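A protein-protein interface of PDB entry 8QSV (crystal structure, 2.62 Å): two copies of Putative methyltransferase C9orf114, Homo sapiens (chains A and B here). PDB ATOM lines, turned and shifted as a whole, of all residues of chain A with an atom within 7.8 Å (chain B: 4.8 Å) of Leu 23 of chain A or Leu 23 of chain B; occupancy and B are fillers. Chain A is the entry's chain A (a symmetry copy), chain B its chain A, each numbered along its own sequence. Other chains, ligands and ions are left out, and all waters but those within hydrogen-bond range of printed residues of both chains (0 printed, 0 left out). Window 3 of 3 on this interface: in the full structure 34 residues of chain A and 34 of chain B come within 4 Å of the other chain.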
ATOM      1  N   ILE A  14     -30.565   5.682   3.801  1.00  0.00           N
ATOM      2  CA  ILE A  14     -29.370   6.001   3.039  1.00  0.00           C
ATOM      3  C   ILE A  14     -28.898   4.785   2.254  1.00  0.00           C
ATOM      4  O   ILE A  14     -28.191   4.956   1.257  1.00  0.00           O
ATOM      5  CB  ILE A  14     -28.213   6.513   3.914  1.00  0.00           C
ATOM      6  CG1 ILE A  14     -27.748   5.469   4.930  1.00  0.00           C
ATOM      7  CG2 ILE A  14     -28.549   7.840   4.567  1.00  0.00           C
ATOM      8  CD1 ILE A  14     -26.476   5.865   5.631  1.00  0.00           C
ATOM      9  N   LEU A  15     -29.301   3.584   2.708  1.00  0.00           N
ATOM     10  CA  LEU A  15     -28.975   2.341   2.018  1.00  0.00           C
ATOM     11  C   LEU A  15     -29.748   2.216   0.723  1.00  0.00           C
ATOM     12  O   LEU A  15     -29.286   1.548  -0.182  1.00  0.00           O
ATOM     13  CB  LEU A  15     -29.224   1.141   2.928  1.00  0.00           C
ATOM     14  CG  LEU A  15     -27.972   0.618   3.626  1.00  0.00           C
ATOM     15  CD1 LEU A  15     -27.299   1.707   4.425  1.00  0.00           C
ATOM     16  CD2 LEU A  15     -28.289  -0.556   4.527  1.00  0.00           C
ATOM     17  N   ASN A  17     -30.091   4.483  -1.353  1.00  0.00           N
ATOM     18  CA  ASN A  17     -29.485   5.405  -2.299  1.00  0.00           C
ATOM     19  C   ASN A  17     -28.358   4.710  -3.064  1.00  0.00           C
ATOM     20  O   ASN A  17     -27.901   5.219  -4.079  1.00  0.00           O
ATOM     21  CB  ASN A  17     -28.974   6.665  -1.589  1.00  0.00           C
ATOM     22  CG  ASN A  17     -30.070   7.583  -1.064  1.00  0.00           C
ATOM     23  OD1 ASN A  17     -29.834   8.399  -0.166  1.00  0.00           O
ATOM     24  ND2 ASN A  17     -31.269   7.464  -1.611  1.00  0.00           N
ATOM     25  N   ALA A  18     -27.905   3.539  -2.604  1.00  0.00           N
ATOM     26  CA  ALA A  18     -26.726   2.928  -3.193  1.00  0.00           C
ATOM     27  C   ALA A  18     -27.023   2.446  -4.605  1.00  0.00           C
ATOM     28  O   ALA A  18     -28.129   2.015  -4.903  1.00  0.00           O
ATOM     29  CB  ALA A  18     -26.252   1.795  -2.330  1.00  0.00           C
ATOM     30  N   GLN A  19     -25.994   2.502  -5.455  1.00  0.00           N
ATOM     31  CA  GLN A  19     -26.070   2.057  -6.838  1.00  0.00           C
ATOM     32  C   GLN A  19     -25.946   0.541  -6.976  1.00  0.00           C
ATOM     33  O   GLN A  19     -26.273   0.029  -8.034  1.00  0.00           O
ATOM     34  CB  GLN A  19     -24.944   2.677  -7.673  1.00  0.00           C
ATOM     35  CG  GLN A  19     -25.367   3.811  -8.600  1.00  0.00           C
ATOM     36  CD  GLN A  19     -25.673   5.062  -7.818  1.00  0.00           C
ATOM     37  OE1 GLN A  19     -25.672   5.061  -6.593  1.00  0.00           O
ATOM     38  NE2 GLN A  19     -25.960   6.142  -8.520  1.00  0.00           N
ATOM     39  N   SER A  20     -25.410  -0.159  -5.966  1.00  0.00           N
ATOM     40  CA  SER A  20     -25.120  -1.589  -6.052  1.00  0.00           C
ATOM     41  C   SER A  20     -25.436  -2.296  -4.743  1.00  0.00           C
ATOM     42  O   SER A  20     -25.314  -1.760  -3.649  1.00  0.00           O
ATOM     43  CB  SER A  20     -23.670  -1.877  -6.326  1.00  0.00           C
ATOM     44  OG  SER A  20     -23.302  -1.446  -7.610  1.00  0.00           O
ATOM     45  N   PRO A  21     -25.714  -3.604  -4.810  1.00  0.00           N
ATOM     46  CA  PRO A  21     -25.725  -4.416  -3.594  1.00  0.00           C
ATOM     47  C   PRO A  21     -24.406  -4.308  -2.832  1.00  0.00           C
ATOM     48  O   PRO A  21     -24.377  -4.168  -1.604  1.00  0.00           O
ATOM     49  CB  PRO A  21     -25.948  -5.833  -4.127  1.00  0.00           C
ATOM     50  CG  PRO A  21     -26.536  -5.661  -5.539  1.00  0.00           C
ATOM     51  CD  PRO A  21     -26.026  -4.337  -6.049  1.00  0.00           C
ATOM     52  N   GLU A  22     -23.297  -4.385  -3.570  1.00  0.00           N
ATOM     53  CA  GLU A  22     -21.987  -4.346  -2.943  1.00  0.00           C
ATOM     54  C   GLU A  22     -21.821  -3.011  -2.200  1.00  0.00           C
ATOM     55  O   GLU A  22     -21.613  -3.003  -0.996  1.00  0.00           O
ATOM     56  CB  GLU A  22     -20.909  -4.614  -3.991  1.00  0.00           C
ATOM     57  CG  GLU A  22     -21.066  -5.951  -4.687  1.00  0.00           C
ATOM     58  CD  GLU A  22     -22.152  -6.062  -5.753  1.00  0.00           C
ATOM     59  OE1 GLU A  22     -22.372  -5.088  -6.509  1.00  0.00           O
ATOM     60  OE2 GLU A  22     -22.743  -7.153  -5.873  1.00  0.00           O
ATOM     61  N   LEU A  23     -22.012  -1.879  -2.886  1.00  0.00           N
ATOM     62  CA  LEU A  23     -21.901  -0.562  -2.263  1.00  0.00           C
ATOM     63  C   LEU A  23     -22.886  -0.324  -1.120  1.00  0.00           C
ATOM     64  O   LEU A  23     -22.614   0.488  -0.235  1.00  0.00           O
ATOM     65  CB  LEU A  23     -22.126   0.495  -3.339  1.00  0.00           C
ATOM     66  CG  LEU A  23     -21.047   0.520  -4.416  1.00  0.00           C
ATOM     67  CD1 LEU A  23     -21.497   1.322  -5.607  1.00  0.00           C
ATOM     68  CD2 LEU A  23     -19.734   1.063  -3.876  1.00  0.00           C
ATOM     69  N   ARG A  24     -24.047  -0.977  -1.155  1.00  0.00           N
ATOM     70  CA  ARG A  24     -25.027  -0.886  -0.081  1.00  0.00           C
ATOM     71  C   ARG A  24     -24.370  -1.425   1.184  1.00  0.00           C
ATOM     72  O   ARG A  24     -24.447  -0.834   2.257  1.00  0.00           O
ATOM     73  CB  ARG A  24     -26.296  -1.632  -0.505  1.00  0.00           C
ATOM     74  CG  ARG A  24     -27.527  -1.502   0.388  1.00  0.00           C
ATOM     75  CD  ARG A  24     -28.650  -2.381  -0.207  1.00  0.00           C
ATOM     76  NE  ARG A  24     -29.862  -2.458   0.609  1.00  0.00           N
ATOM     77  CZ  ARG A  24     -30.824  -1.531   0.662  1.00  0.00           C
ATOM     78  NH1 ARG A  24     -31.049  -0.724  -0.360  1.00  0.00           N
ATOM     79  NH2 ARG A  24     -31.621  -1.470   1.716  1.00  0.00           N
ATOM     80  N   THR A  25     -23.631  -2.513   1.025  1.00  0.00           N
ATOM     81  CA  THR A  25     -22.937  -3.124   2.141  1.00  0.00           C
ATOM     82  C   THR A  25     -21.785  -2.238   2.576  1.00  0.00           C
ATOM     83  O   THR A  25     -21.617  -2.021   3.771  1.00  0.00           O
ATOM     84  CB  THR A  25     -22.399  -4.502   1.753  1.00  0.00           C
ATOM     85  OG1 THR A  25     -23.500  -5.354   1.451  1.00  0.00           O
ATOM     86  CG2 THR A  25     -21.592  -5.136   2.852  1.00  0.00           C
ATOM     87  N   TYR A  26     -20.971  -1.786   1.612  1.00  0.00           N
ATOM     88  CA  TYR A  26     -19.822  -0.953   1.926  1.00  0.00           C
ATOM     89  C   TYR A  26     -20.286   0.292   2.683  1.00  0.00           C
ATOM     90  O   TYR A  26     -19.719   0.685   3.713  1.00  0.00           O
ATOM     91  CB  TYR A  26     -19.034  -0.664   0.646  1.00  0.00           C
ATOM     92  CG  TYR A  26     -17.712   0.052   0.809  1.00  0.00           C
ATOM     93  CD1 TYR A  26     -17.658   1.433   0.837  1.00  0.00           C
ATOM     94  CD2 TYR A  26     -16.514  -0.650   0.893  1.00  0.00           C
ATOM     95  CE1 TYR A  26     -16.452   2.096   0.948  1.00  0.00           C
ATOM     96  CE2 TYR A  26     -15.299  -0.004   1.034  1.00  0.00           C
ATOM     97  CZ  TYR A  26     -15.266   1.381   1.053  1.00  0.00           C
ATOM     98  OH  TYR A  26     -14.085   2.093   1.167  1.00  0.00           O
ATOM     99  N   LEU A  27     -21.384   0.883   2.221  1.00  0.00           N
ATOM    100  CA  LEU A  27     -21.840   2.083   2.886  1.00  0.00           C
ATOM    101  C   LEU A  27     -22.125   1.767   4.359  1.00  0.00           C
ATOM    102  O   LEU A  27     -21.799   2.541   5.263  1.00  0.00           O
ATOM    103  CB  LEU A  27     -23.054   2.638   2.142  1.00  0.00           C
ATOM    104  CG  LEU A  27     -23.702   3.840   2.831  1.00  0.00           C
ATOM    105  CD1 LEU A  27     -22.759   5.026   2.828  1.00  0.00           C
ATOM    106  CD2 LEU A  27     -25.024   4.211   2.167  1.00  0.00           C
ATOM    107  N   ALA A  28     -22.737   0.608   4.617  1.00  0.00           N
ATOM    108  CA  ALA A  28     -23.056   0.243   5.989  1.00  0.00           C
ATOM    109  C   ALA A  28     -21.778   0.215   6.823  1.00  0.00           C
ATOM    110  O   ALA A  28     -21.731   0.761   7.920  1.00  0.00           O
ATOM    111  CB  ALA A  28     -23.711  -1.092   5.991  1.00  0.00           C
ATOM    112  N   GLY A  29     -20.734  -0.404   6.260  1.00  0.00           N
ATOM    113  CA  GLY A  29     -19.408  -0.426   6.851  1.00  0.00           C
ATOM    114  C   GLY A  29     -18.857   0.974   7.126  1.00  0.00           C
ATOM    115  O   GLY A  29     -18.286   1.251   8.199  1.00  0.00           O
ATOM    116  N   GLN A  30     -19.030   1.874   6.154  1.00  0.00           N
ATOM    117  CA  GLN A  30     -18.489   3.219   6.331  1.00  0.00           C
ATOM    118  C   GLN A  30     -19.044   3.790   7.617  1.00  0.00           C
ATOM    119  O   GLN A  30     -18.276   4.376   8.366  1.00  0.00           O
ATOM    120  CB  GLN A  30     -18.789   4.149   5.159  1.00  0.00           C
ATOM    121  CG  GLN A  30     -18.216   3.635   3.846  1.00  0.00           C
ATOM    122  CD  GLN A  30     -18.538   4.563   2.716  1.00  0.00           C
ATOM    123  OE1 GLN A  30     -19.275   4.224   1.782  1.00  0.00           O
ATOM    124  NE2 GLN A  30     -17.944   5.744   2.792  1.00  0.00           N
ATOM    125  N   PHE A  99     -22.497  -9.794   1.594  1.00  0.00           N
ATOM    126  CA  PHE A  99     -21.283  -9.071   1.261  1.00  0.00           C
ATOM    127  C   PHE A  99     -20.477  -8.755   2.523  1.00  0.00           C
ATOM    128  O   PHE A  99     -19.749  -7.767   2.550  1.00  0.00           O
ATOM    129  CB  PHE A  99     -21.654  -7.807   0.483  1.00  0.00           C
ATOM    130  CG  PHE A  99     -22.496  -8.044  -0.742  1.00  0.00           C
ATOM    131  CD1 PHE A  99     -21.989  -8.753  -1.828  1.00  0.00           C
ATOM    132  CD2 PHE A  99     -23.795  -7.563  -0.812  1.00  0.00           C
ATOM    133  CE1 PHE A  99     -22.759  -8.981  -2.961  1.00  0.00           C
ATOM    134  CE2 PHE A  99     -24.563  -7.783  -1.946  1.00  0.00           C
ATOM    135  CZ  PHE A  99     -24.048  -8.497  -3.014  1.00  0.00           C
ATOM    136  N   GLY A 101     -17.858 -10.066   3.335  1.00  0.00           N
ATOM    137  CA  GLY A 101     -16.517 -10.094   2.776  1.00  0.00           C
ATOM    138  C   GLY A 101     -15.962  -8.709   2.486  1.00  0.00           C
ATOM    139  O   GLY A 101     -14.991  -8.307   3.123  1.00  0.00           O
ATOM    140  N   LEU A 102     -16.627  -7.982   1.572  1.00  0.00           N
ATOM    141  CA  LEU A 102     -16.145  -6.717   1.007  1.00  0.00           C
ATOM    142  C   LEU A 102     -16.247  -5.568   2.017  1.00  0.00           C
ATOM    143  O   LEU A 102     -16.489  -4.415   1.645  1.00  0.00           O
ATOM    144  CB  LEU A 102     -16.959  -6.373  -0.251  1.00  0.00           C
ATOM    145  CG  LEU A 102     -17.138  -7.488  -1.276  1.00  0.00           C
ATOM    146  CD1 LEU A 102     -17.512  -6.883  -2.619  1.00  0.00           C
ATOM    147  CD2 LEU A 102     -15.884  -8.359  -1.386  1.00  0.00           C
ATOM    148  N   LEU A 103     -16.049  -5.900   3.296  1.00  0.00           N
ATOM    149  CA  LEU A 103     -16.106  -4.915   4.353  1.00  0.00           C
ATOM    150  C   LEU A 103     -14.687  -4.521   4.728  1.00  0.00           C
ATOM    151  O   LEU A 103     -13.761  -5.323   4.618  1.00  0.00           O
ATOM    152  CB  LEU A 103     -16.860  -5.466   5.580  1.00  0.00           C
ATOM    153  CG  LEU A 103     -18.329  -5.054   5.749  1.00  0.00           C
ATOM    154  CD1 LEU A 103     -18.674  -3.746   5.007  1.00  0.00           C
ATOM    155  CD2 LEU A 103     -19.257  -6.186   5.334  1.00  0.00           C
ATOM    156  N   ASN A 104     -14.592  -3.236   5.050  1.00  0.00           N
ATOM    157  CA  ASN A 104     -13.772  -2.641   6.091  1.00  0.00           C
ATOM    158  C   ASN A 104     -14.013  -3.153   7.526  1.00  0.00           C
ATOM    159  O   ASN A 104     -15.045  -2.876   8.152  1.00  0.00           O
ATOM    160  CB  ASN A 104     -14.062  -1.133   6.132  1.00  0.00           C
ATOM    161  CG  ASN A 104     -15.515  -0.718   5.908  1.00  0.00           C
ATOM    162  OD1 ASN A 104     -15.798   0.216   5.155  1.00  0.00           O
ATOM    163  ND2 ASN A 104     -16.444  -1.357   6.600  1.00  0.00           N
ATOM    164  N   ALA B  18      -7.927  -1.787  -2.623  1.00  0.00           N
ATOM    165  CA  ALA B  18      -9.342  -2.061  -2.800  1.00  0.00           C
ATOM    166  C   ALA B  18      -9.570  -3.539  -3.081  1.00  0.00           C
ATOM    167  O   ALA B  18      -8.753  -4.190  -3.719  1.00  0.00           O
ATOM    168  CB  ALA B  18      -9.893  -1.214  -3.910  1.00  0.00           C
ATOM    169  N   GLN B  19     -10.717  -4.038  -2.615  1.00  0.00           N
ATOM    170  CA  GLN B  19     -11.129  -5.420  -2.811  1.00  0.00           C
ATOM    171  C   GLN B  19     -11.725  -5.666  -4.195  1.00  0.00           C
ATOM    172  O   GLN B  19     -11.843  -6.818  -4.576  1.00  0.00           O
ATOM    173  CB  GLN B  19     -12.197  -5.820  -1.786  1.00  0.00           C
ATOM    174  CG  GLN B  19     -11.709  -6.713  -0.650  1.00  0.00           C
ATOM    175  CD  GLN B  19     -10.861  -5.935   0.322  1.00  0.00           C
ATOM    176  OE1 GLN B  19     -10.551  -4.770   0.103  1.00  0.00           O
ATOM    177  NE2 GLN B  19     -10.458  -6.579   1.400  1.00  0.00           N
ATOM    178  N   SER B  20     -12.168  -4.618  -4.904  1.00  0.00           N
ATOM    179  CA  SER B  20     -12.878  -4.756  -6.175  1.00  0.00           C
ATOM    180  C   SER B  20     -12.461  -3.676  -7.161  1.00  0.00           C
ATOM    181  O   SER B  20     -12.138  -2.546  -6.815  1.00  0.00           O
ATOM    182  CB  SER B  20     -14.368  -4.620  -6.031  1.00  0.00           C
ATOM    183  OG  SER B  20     -14.906  -5.689  -5.298  1.00  0.00           O
ATOM    184  N   PRO B  21     -12.607  -3.952  -8.462  1.00  0.00           N
ATOM    185  CA  PRO B  21     -12.527  -2.880  -9.454  1.00  0.00           C
ATOM    186  C   PRO B  21     -13.516  -1.757  -9.153  1.00  0.00           C
ATOM    187  O   PRO B  21     -13.189  -0.567  -9.231  1.00  0.00           O
ATOM    188  CB  PRO B  21     -12.873  -3.594 -10.763  1.00  0.00           C
ATOM    189  CG  PRO B  21     -12.640  -5.092 -10.497  1.00  0.00           C
ATOM    190  CD  PRO B  21     -12.850  -5.294  -9.017  1.00  0.00           C
ATOM    191  N   GLU B  22     -14.748  -2.140  -8.812  1.00  0.00           N
ATOM    192  CA  GLU B  22     -15.785  -1.155  -8.554  1.00  0.00           C
ATOM    193  C   GLU B  22     -15.356  -0.267  -7.375  1.00  0.00           C
ATOM    194  O   GLU B  22     -15.240   0.939  -7.529  1.00  0.00           O
ATOM    195  CB  GLU B  22     -17.122  -1.861  -8.347  1.00  0.00           C
ATOM    196  CG  GLU B  22     -17.548  -2.702  -9.534  1.00  0.00           C
ATOM    197  CD  GLU B  22     -16.851  -4.046  -9.725  1.00  0.00           C
ATOM    198  OE1 GLU B  22     -16.554  -4.732  -8.721  1.00  0.00           O
ATOM    199  OE2 GLU B  22     -16.658  -4.442 -10.891  1.00  0.00           O
ATOM    200  N   LEU B  23     -15.022  -0.863  -6.225  1.00  0.00           N
ATOM    201  CA  LEU B  23     -14.578  -0.106  -5.056  1.00  0.00           C
ATOM    202  C   LEU B  23     -13.310   0.715  -5.284  1.00  0.00           C
ATOM    203  O   LEU B  23     -13.097   1.716  -4.601  1.00  0.00           O
ATOM    204  CB  LEU B  23     -14.333  -1.090  -3.917  1.00  0.00           C
ATOM    205  CG  LEU B  23     -15.594  -1.794  -3.426  1.00  0.00           C
ATOM    206  CD1 LEU B  23     -15.246  -2.978  -2.566  1.00  0.00           C
ATOM    207  CD2 LEU B  23     -16.507  -0.840  -2.673  1.00  0.00           C
ATOM    208  N   ARG B  24     -12.441   0.275  -6.194  1.00  0.00           N
ATOM    209  CA  ARG B  24     -11.238   1.017  -6.547  1.00  0.00           C
ATOM    210  C   ARG B  24     -11.681   2.358  -7.119  1.00  0.00           C
ATOM    211  O   ARG B  24     -11.163   3.415  -6.768  1.00  0.00           O
ATOM    212  CB  ARG B  24     -10.397   0.166  -7.504  1.00  0.00           C
ATOM    213  CG  ARG B  24      -8.997   0.666  -7.852  1.00  0.00           C
ATOM    214  CD  ARG B  24      -8.372  -0.318  -8.867  1.00  0.00           C
ATOM    215  NE  ARG B  24      -7.071   0.094  -9.394  1.00  0.00           N
ATOM    216  CZ  ARG B  24      -5.898  -0.046  -8.767  1.00  0.00           C
ATOM    217  NH1 ARG B  24      -5.713  -1.004  -7.874  1.00  0.00           N
ATOM    218  NH2 ARG B  24      -4.878   0.727  -9.100  1.00  0.00           N
ATOM    219  N   THR B  25     -12.722   2.316  -7.937  1.00  0.00           N
ATOM    220  CA  THR B  25     -13.257   3.520  -8.540  1.00  0.00           C
ATOM    221  C   THR B  25     -13.948   4.361  -7.483  1.00  0.00           C
ATOM    222  O   THR B  25     -13.735   5.567  -7.447  1.00  0.00           O
ATOM    223  CB  THR B  25     -14.257   3.172  -9.644  1.00  0.00           C
ATOM    224  OG1 THR B  25     -13.570   2.476 -10.680  1.00  0.00           O
ATOM    225  CG2 THR B  25     -14.907   4.391 -10.238  1.00  0.00           C
ATOM    226  N   TYR B  26     -14.809   3.729  -6.674  1.00  0.00           N
ATOM    227  CA  TYR B  26     -15.544   4.448  -5.647  1.00  0.00           C
ATOM    228  C   TYR B  26     -14.557   5.156  -4.716  1.00  0.00           C
ATOM    229  O   TYR B  26     -14.703   6.341  -4.382  1.00  0.00           O
ATOM    230  CB  TYR B  26     -16.510   3.493  -4.943  1.00  0.00           C
ATOM    231  CG  TYR B  26     -17.476   4.107  -3.956  1.00  0.00           C
ATOM    232  CD1 TYR B  26     -17.113   4.288  -2.634  1.00  0.00           C
ATOM    233  CD2 TYR B  26     -18.765   4.470  -4.334  1.00  0.00           C
ATOM    234  CE1 TYR B  26     -18.001   4.814  -1.717  1.00  0.00           C
ATOM    235  CE2 TYR B  26     -19.659   5.026  -3.435  1.00  0.00           C
ATOM    236  CZ  TYR B  26     -19.276   5.191  -2.114  1.00  0.00           C
ATOM    237  OH  TYR B  26     -20.126   5.717  -1.157  1.00  0.00           O
ATOM    238  N   LEU B  27     -13.489   4.452  -4.351  1.00  0.00           N
ATOM    239  CA  LEU B  27     -12.547   5.070  -3.445  1.00  0.00           C
ATOM    240  C   LEU B  27     -12.004   6.355  -4.080  1.00  0.00           C
ATOM    241  O   LEU B  27     -11.846   7.387  -3.423  1.00  0.00           O
ATOM    242  CB  LEU B  27     -11.455   4.062  -3.093  1.00  0.00           C
ATOM    243  CG  LEU B  27     -10.329   4.645  -2.238  1.00  0.00           C
ATOM    244  CD1 LEU B  27     -10.850   5.038  -0.870  1.00  0.00           C
ATOM    245  CD2 LEU B  27      -9.171   3.663  -2.103  1.00  0.00           C
ATOM    246  N   LEU B 102     -20.644   4.350 -11.452  1.00  0.00           N
ATOM    247  CA  LEU B 102     -20.860   4.081 -10.027  1.00  0.00           C
ATOM    248  C   LEU B 102     -20.172   5.126  -9.140  1.00  0.00           C
ATOM    249  O   LEU B 102     -19.705   4.816  -8.040  1.00  0.00           O
ATOM    250  CB  LEU B 102     -20.329   2.681  -9.683  1.00  0.00           C
ATOM    251  CG  LEU B 102     -20.753   1.543 -10.604  1.00  0.00           C
ATOM    252  CD1 LEU B 102     -20.571   0.216  -9.885  1.00  0.00           C
ATOM    253  CD2 LEU B 102     -22.192   1.720 -11.094  1.00  0.00           C
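OH of Tyr 26 of chain B lies within hydrogen-bond range of OE1 of Gln 30 of chain A.
Among the printed residues, pairs that only touch across the chains: Ser 20 of chain A with Leu 102 of chain B (3.9 Å), Leu 23 of chain A with Leu 23 of chain B (3.9 Å), Leu 23 of chain A with Tyr 26 of chain B (3.6 Å), Tyr 26 of chain A with Leu 23 of chain B (3.6 Å) and Leu 102 of chain A with Ser 20 of chain B (3.9 Å).
Of the printed residues of chain B, Ser 20 of chain A touches Leu 102. Printed residues of chain B within 4 Å of Tyr 26 of chain A: Leu 23. Printed residues of chain B within 4 Å of Leu 102 of chain A: Ser 20 (3.9 Å). Printed residues of chain A within 4 Å of Ser 20 of chain B: Leu 102. Leu 23 of chain B touches just these residues of chain A: Leu 23 (3.9 Å) and Tyr 26 (3.6 Å). Printed residues of chain A within 4 Å of Tyr 26 of chain B: Leu 23 and Gln 30. The nearest residue of chain B that does not touch Leu 23 of chain A is Leu 102 of chain B (4.5 Å).
Of the 11 printed residues of chain B, 4 touch a printed residue of chain A. Printed residues of chain B that touch a printed residue of chain A: Ser 20, Leu 23, Tyr 26 and Leu 102. Hydrophobic or aromatic side chains of chain B within 4 Å of the printed part of chain A: Leu 23, Tyr 26 and Leu 102. Among the printed residues, 6 pairs touch across the chains. Among the printed residues, no Asp or Glu carboxylate lies within 4 Å of a Lys or Arg side-chain nitrogen of the other chain.
Ser 20 of chain A touches Leu 102 of chain B, and with the chains exchanged Leu 102 of chain A touches Ser 20 of chain B. Leu 23 of chain B touches its own counterpart, Leu 23 of chain A. Leu 23 of chain A touches Tyr 26 of chain B, and with the chains exchanged Tyr 26 of chain A touches Leu 23 of chain B. 11 positions are printed for both chains. Of the 6 pairs that touch across the chains among the printed residues, 5 have their exchanged pair printed and touching as well.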
